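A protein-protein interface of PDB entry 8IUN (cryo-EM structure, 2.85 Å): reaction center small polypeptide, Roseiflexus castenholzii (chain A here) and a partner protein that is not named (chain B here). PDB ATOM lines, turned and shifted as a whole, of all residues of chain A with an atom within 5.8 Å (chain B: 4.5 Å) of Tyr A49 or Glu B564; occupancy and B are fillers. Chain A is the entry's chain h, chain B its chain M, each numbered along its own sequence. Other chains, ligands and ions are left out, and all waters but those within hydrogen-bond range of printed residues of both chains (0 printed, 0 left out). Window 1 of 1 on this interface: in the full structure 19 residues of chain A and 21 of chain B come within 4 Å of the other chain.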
ATOM      1  N   GLN A  44      -3.154  -6.396  11.671  1.00  0.00           N
ATOM      2  CA  GLN A  44      -2.977  -6.747  10.266  1.00  0.00           C
ATOM      3  C   GLN A  44      -2.034  -5.789   9.554  1.00  0.00           C
ATOM      4  O   GLN A  44      -1.221  -6.221   8.733  1.00  0.00           O
ATOM      5  CB  GLN A  44      -4.331  -6.769   9.561  1.00  0.00           C
ATOM      6  CG  GLN A  44      -4.555  -7.965   8.657  1.00  0.00           C
ATOM      7  CD  GLN A  44      -3.854  -7.848   7.322  1.00  0.00           C
ATOM      8  OE1 GLN A  44      -4.154  -6.955   6.532  1.00  0.00           O
ATOM      9  NE2 GLN A  44      -2.926  -8.758   7.056  1.00  0.00           N
ATOM     10  N   ALA A  45      -2.121  -4.492   9.851  1.00  0.00           N
ATOM     11  CA  ALA A  45      -1.390  -3.500   9.072  1.00  0.00           C
ATOM     12  C   ALA A  45       0.105  -3.477   9.373  1.00  0.00           C
ATOM     13  O   ALA A  45       0.897  -3.122   8.495  1.00  0.00           O
ATOM     14  CB  ALA A  45      -1.991  -2.117   9.307  1.00  0.00           C
ATOM     15  N   THR A  46       0.517  -3.830  10.591  1.00  0.00           N
ATOM     16  CA  THR A  46       1.919  -3.742  10.990  1.00  0.00           C
ATOM     17  C   THR A  46       2.643  -5.081  10.932  1.00  0.00           C
ATOM     18  O   THR A  46       3.629  -5.275  11.653  1.00  0.00           O
ATOM     19  CB  THR A  46       2.033  -3.150  12.394  1.00  0.00           C
ATOM     20  OG1 THR A  46       1.256  -3.934  13.303  1.00  0.00           O
ATOM     21  CG2 THR A  46       1.533  -1.726  12.420  1.00  0.00           C
ATOM     22  N   SER A  47       2.192  -6.010  10.097  1.00  0.00           N
ATOM     23  CA  SER A  47       2.847  -7.303   9.976  1.00  0.00           C
ATOM     24  C   SER A  47       3.843  -7.269   8.816  1.00  0.00           C
ATOM     25  O   SER A  47       4.094  -6.224   8.212  1.00  0.00           O
ATOM     26  CB  SER A  47       1.807  -8.408   9.817  1.00  0.00           C
ATOM     27  OG  SER A  47       1.021  -8.215   8.663  1.00  0.00           O
ATOM     28  N   ALA A  48       4.429  -8.419   8.498  1.00  0.00           N
ATOM     29  CA  ALA A  48       5.448  -8.532   7.462  1.00  0.00           C
ATOM     30  C   ALA A  48       4.822  -9.118   6.206  1.00  0.00           C
ATOM     31  O   ALA A  48       4.276 -10.224   6.239  1.00  0.00           O
ATOM     32  CB  ALA A  48       6.614  -9.399   7.934  1.00  0.00           C
ATOM     33  N   TYR A  49       4.903  -8.375   5.107  1.00  0.00           N
ATOM     34  CA  TYR A  49       4.395  -8.825   3.822  1.00  0.00           C
ATOM     35  C   TYR A  49       5.153  -8.085   2.727  1.00  0.00           C
ATOM     36  O   TYR A  49       6.124  -7.375   2.996  1.00  0.00           O
ATOM     37  CB  TYR A  49       2.874  -8.642   3.738  1.00  0.00           C
ATOM     38  CG  TYR A  49       2.334  -7.282   4.124  1.00  0.00           C
ATOM     39  CD1 TYR A  49       2.501  -6.184   3.297  1.00  0.00           C
ATOM     40  CD2 TYR A  49       1.608  -7.114   5.289  1.00  0.00           C
ATOM     41  CE1 TYR A  49       1.993  -4.958   3.635  1.00  0.00           C
ATOM     42  CE2 TYR A  49       1.096  -5.891   5.634  1.00  0.00           C
ATOM     43  CZ  TYR A  49       1.292  -4.819   4.805  1.00  0.00           C
ATOM     44  OH  TYR A  49       0.782  -3.594   5.144  1.00  0.00           O
ATOM     45  N   LEU A  50       4.710  -8.254   1.485  1.00  0.00           N
ATOM     46  CA  LEU A  50       5.454  -7.738   0.341  1.00  0.00           C
ATOM     47  C   LEU A  50       5.419  -6.216   0.317  1.00  0.00           C
ATOM     48  O   LEU A  50       4.346  -5.610   0.246  1.00  0.00           O
ATOM     49  CB  LEU A  50       4.887  -8.297  -0.961  1.00  0.00           C
ATOM     50  CG  LEU A  50       5.132  -9.771  -1.272  1.00  0.00           C
ATOM     51  CD1 LEU A  50       4.511 -10.118  -2.600  1.00  0.00           C
ATOM     52  CD2 LEU A  50       6.609 -10.075  -1.289  1.00  0.00           C
ATOM     53  N   ARG A  51       6.598  -5.601   0.365  1.00  0.00           N
ATOM     54  CA  ARG A  51       6.744  -4.159   0.271  1.00  0.00           C
ATOM     55  C   ARG A  51       7.907  -3.848  -0.656  1.00  0.00           C
ATOM     56  O   ARG A  51       8.820  -4.658  -0.818  1.00  0.00           O
ATOM     57  CB  ARG A  51       7.001  -3.512   1.639  1.00  0.00           C
ATOM     58  CG  ARG A  51       5.894  -3.669   2.653  1.00  0.00           C
ATOM     59  CD  ARG A  51       6.312  -3.076   3.982  1.00  0.00           C
ATOM     60  NE  ARG A  51       5.204  -2.956   4.922  1.00  0.00           N
ATOM     61  CZ  ARG A  51       4.956  -3.808   5.904  1.00  0.00           C
ATOM     62  NH1 ARG A  51       5.712  -4.872   6.104  1.00  0.00           N
ATOM     63  NH2 ARG A  51       3.926  -3.582   6.711  1.00  0.00           N
ATOM     64  N   LEU A  52       7.868  -2.669  -1.266  1.00  0.00           N
ATOM     65  CA  LEU A  52       9.017  -2.184  -2.010  1.00  0.00           C
ATOM     66  C   LEU A  52      10.076  -1.665  -1.048  1.00  0.00           C
ATOM     67  O   LEU A  52       9.765  -1.138   0.024  1.00  0.00           O
ATOM     68  CB  LEU A  52       8.607  -1.086  -2.990  1.00  0.00           C
ATOM     69  CG  LEU A  52       7.653  -1.491  -4.112  1.00  0.00           C
ATOM     70  CD1 LEU A  52       7.348  -0.310  -5.004  1.00  0.00           C
ATOM     71  CD2 LEU A  52       8.227  -2.624  -4.926  1.00  0.00           C
ATOM     72  N   GLU B 560      -1.362  -1.504  -5.229  1.00  0.00           N
ATOM     73  CA  GLU B 560      -0.821  -1.360  -3.886  1.00  0.00           C
ATOM     74  C   GLU B 560      -1.224  -2.502  -2.970  1.00  0.00           C
ATOM     75  O   GLU B 560      -0.543  -2.744  -1.971  1.00  0.00           O
ATOM     76  CB  GLU B 560      -1.268  -0.034  -3.272  1.00  0.00           C
ATOM     77  CG  GLU B 560      -0.775   1.187  -4.014  1.00  0.00           C
ATOM     78  CD  GLU B 560       0.694   1.464  -3.777  1.00  0.00           C
ATOM     79  OE1 GLU B 560       1.130   1.402  -2.613  1.00  0.00           O
ATOM     80  OE2 GLU B 560       1.412   1.749  -4.755  1.00  0.00           O
ATOM     81  N   ALA B 563       1.802  -5.094  -3.536  1.00  0.00           N
ATOM     82  CA  ALA B 563       3.089  -4.720  -2.952  1.00  0.00           C
ATOM     83  C   ALA B 563       3.066  -3.222  -2.702  1.00  0.00           C
ATOM     84  O   ALA B 563       2.870  -2.448  -3.642  1.00  0.00           O
ATOM     85  CB  ALA B 563       4.247  -5.096  -3.868  1.00  0.00           C
ATOM     86  N   GLU B 564       3.273  -2.814  -1.453  1.00  0.00           N
ATOM     87  CA  GLU B 564       3.114  -1.423  -1.053  1.00  0.00           C
ATOM     88  C   GLU B 564       4.385  -0.618  -1.284  1.00  0.00           C
ATOM     89  O   GLU B 564       5.489  -1.073  -0.977  1.00  0.00           O
ATOM     90  CB  GLU B 564       2.711  -1.336   0.416  1.00  0.00           C
ATOM     91  CG  GLU B 564       1.314  -1.823   0.688  1.00  0.00           C
ATOM     92  CD  GLU B 564       0.868  -1.515   2.092  1.00  0.00           C
ATOM     93  OE1 GLU B 564       1.712  -1.066   2.893  1.00  0.00           O
ATOM     94  OE2 GLU B 564      -0.325  -1.715   2.394  1.00  0.00           O
ATOM     95  N   GLY B 565       4.216   0.592  -1.812  1.00  0.00           N
ATOM     96  CA  GLY B 565       5.323   1.465  -2.118  1.00  0.00           C
ATOM     97  C   GLY B 565       5.422   2.645  -1.174  1.00  0.00           C
ATOM     98  O   GLY B 565       4.764   2.690  -0.133  1.00  0.00           O
ATOM     99  N   THR B 568       2.088   4.635   0.346  1.00  0.00           N
ATOM    100  CA  THR B 568       1.330   3.927   1.371  1.00  0.00           C
ATOM    101  C   THR B 568       2.112   3.850   2.675  1.00  0.00           C
ATOM    102  O   THR B 568       1.537   3.982   3.762  1.00  0.00           O
ATOM    103  CB  THR B 568       0.964   2.528   0.882  1.00  0.00           C
ATOM    104  OG1 THR B 568       0.362   2.620  -0.411  1.00  0.00           O
ATOM    105  CG2 THR B 568      -0.017   1.877   1.832  1.00  0.00           C
ATOM    106  N   GLN B 569       3.424   3.636   2.585  1.00  0.00           N
ATOM    107  CA  GLN B 569       4.260   3.613   3.780  1.00  0.00           C
ATOM    108  C   GLN B 569       4.223   4.953   4.502  1.00  0.00           C
ATOM    109  O   GLN B 569       4.131   5.002   5.735  1.00  0.00           O
ATOM    110  CB  GLN B 569       5.691   3.241   3.398  1.00  0.00           C
ATOM    111  CG  GLN B 569       5.827   1.871   2.749  1.00  0.00           C
ATOM    112  CD  GLN B 569       7.191   1.642   2.132  1.00  0.00           C
ATOM    113  OE1 GLN B 569       8.037   2.526   2.138  1.00  0.00           O
ATOM    114  NE2 GLN B 569       7.409   0.452   1.599  1.00  0.00           N
ATOM    115  N   GLN B 572       0.825   5.316   6.274  1.00  0.00           N
ATOM    116  CA  GLN B 572       0.812   4.505   7.485  1.00  0.00           C
ATOM    117  C   GLN B 572       1.597   5.172   8.605  1.00  0.00           C
ATOM    118  O   GLN B 572       1.134   5.233   9.749  1.00  0.00           O
ATOM    119  CB  GLN B 572       1.382   3.121   7.189  1.00  0.00           C
ATOM    120  CG  GLN B 572       0.541   2.280   6.263  1.00  0.00           C
ATOM    121  CD  GLN B 572       1.027   0.857   6.184  1.00  0.00           C
ATOM    122  OE1 GLN B 572       2.097   0.581   5.651  1.00  0.00           O
ATOM    123  NE2 GLN B 572       0.246  -0.059   6.727  1.00  0.00           N
ATOM    124  N   ASN B 584      -4.352  -0.364   6.566  1.00  0.00           N
ATOM    125  CA  ASN B 584      -3.737  -0.857   5.346  1.00  0.00           C
ATOM    126  C   ASN B 584      -4.325  -0.139   4.139  1.00  0.00           C
ATOM    127  O   ASN B 584      -5.244   0.671   4.249  1.00  0.00           O
ATOM    128  CB  ASN B 584      -3.966  -2.363   5.218  1.00  0.00           C
ATOM    129  CG  ASN B 584      -2.702  -3.132   5.005  1.00  0.00           C
ATOM    130  OD1 ASN B 584      -1.643  -2.559   4.772  1.00  0.00           O
ATOM    131  ND2 ASN B 584      -2.804  -4.447   5.077  1.00  0.00           N
ATOM    132  N   SER B 585      -3.809  -0.470   2.963  1.00  0.00           N
ATOM    133  CA  SER B 585      -4.454  -0.093   1.714  1.00  0.00           C
ATOM    134  C   SER B 585      -5.605  -1.020   1.360  1.00  0.00           C
ATOM    135  O   SER B 585      -6.241  -0.831   0.321  1.00  0.00           O
ATOM    136  CB  SER B 585      -3.437  -0.069   0.574  1.00  0.00           C
ATOM    137  OG  SER B 585      -2.729  -1.290   0.499  1.00  0.00           O
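Tyr A49 touches just these residues of chain B: Glu B564, Gln B572 and Asn B584.
Glu B564 touches just these residues of chain A: Tyr A49, Leu A50, Arg A51 and Leu A52.
Printed residues of chain B within 4 Å of Leu A50: Ala B563 and Glu B564.
Of the printed residues of chain B, Gln A44 touches Asn B584 (3.2 Å).
Printed residues of chain A within 4 Å of Asn B584: Gln A44 and Tyr A49.
Of the printed residues of chain B, Arg A51 touches Glu B564 and Gln B569.
Printed residues of chain B within 4 Å of Leu A52: Glu B564, Gly B565 and Gln B569.
Thr A46 touches none of the printed residues of chain B.
The backbone NH (N) of Glu B564 is in hydrogen-bond range of the backbone carbonyl oxygen (O) of Leu A50 (3.4 Å).
N of Leu A52 lies within hydrogen-bond range of O of Glu B564 (2.9 Å).
The backbone carbonyl oxygen (O) of Leu A52 sits at hydrogen-bond distance from the side-chain amide nitrogen (NE2) of Gln B569 (3.2 Å).
OE1 of Gln A44 sits at hydrogen-bond distance from ND2 of Asn B584 (3.2 Å).
The side-chain amide oxygen of Asn B584 sits at hydrogen-bond distance from the side-chain hydroxyl of Tyr A49 (2.7 Å).
Of the 9 printed residues of chain B, 6 touch a printed residue of chain A.
Printed residues of chain B that touch a printed residue of chain A: Ala B563, Glu B564, Gly B565, Gln B569, Gln B572 and Asn B584.
Along chain B the printed residues that touch a printed residue of chain A span positions 563 to 584.
Of the 9 printed residues of chain A, 6 touch a printed residue of chain B.
Along chain A the printed residues that touch a printed residue of chain B span positions 44 to 52.
Among the printed residues, no Asp or Glu carboxylate lies within 4 Å of a Lys or Arg side-chain nitrogen of the other chain.
Among the printed residues, merely in contact across the chains: Tyr A49 with Glu B564 (3.5 Å), Leu A50 with Ala B563 (3.5 Å), Arg A51 with Glu B564 (3.6 Å), Ala A45 with Gln B572 (3.6 Å), Tyr A49 with Gln B572 (3.9 Å), Leu A52 with Gly B565 (3.9 Å) and Arg A51 with Gln B569 (3.99 Å).
The side-chain amide oxygen (OE1) of Gln B572 sits close to the side-chain carboxylate (OE1) of Glu B564 (3.2 Å).
The side-chain carboxylate of Glu B564 lies close to the side-chain amide oxygen of Asn B584 (2.8 Å).
The side-chain carboxylate (OE2) of Glu B564 is in hydrogen-bond range of the side-chain hydroxyl (OG) of Ser B585 (3.1 Å).
The backbone carbonyl oxygen (O) of Gln A44 sits at hydrogen-bond distance from the side-chain hydroxyl (OG) of Ser A47 (3.0 Å).
The side-chain hydroxyl (OH) of Tyr A49 lies within hydrogen-bond range of the backbone carbonyl oxygen (O) of Ala A45 (3.4 Å).
The guanidinium group (NH1) of Arg A51 lies within hydrogen-bond range of the backbone carbonyl oxygen (O) of Ser A47 (3.0 Å).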
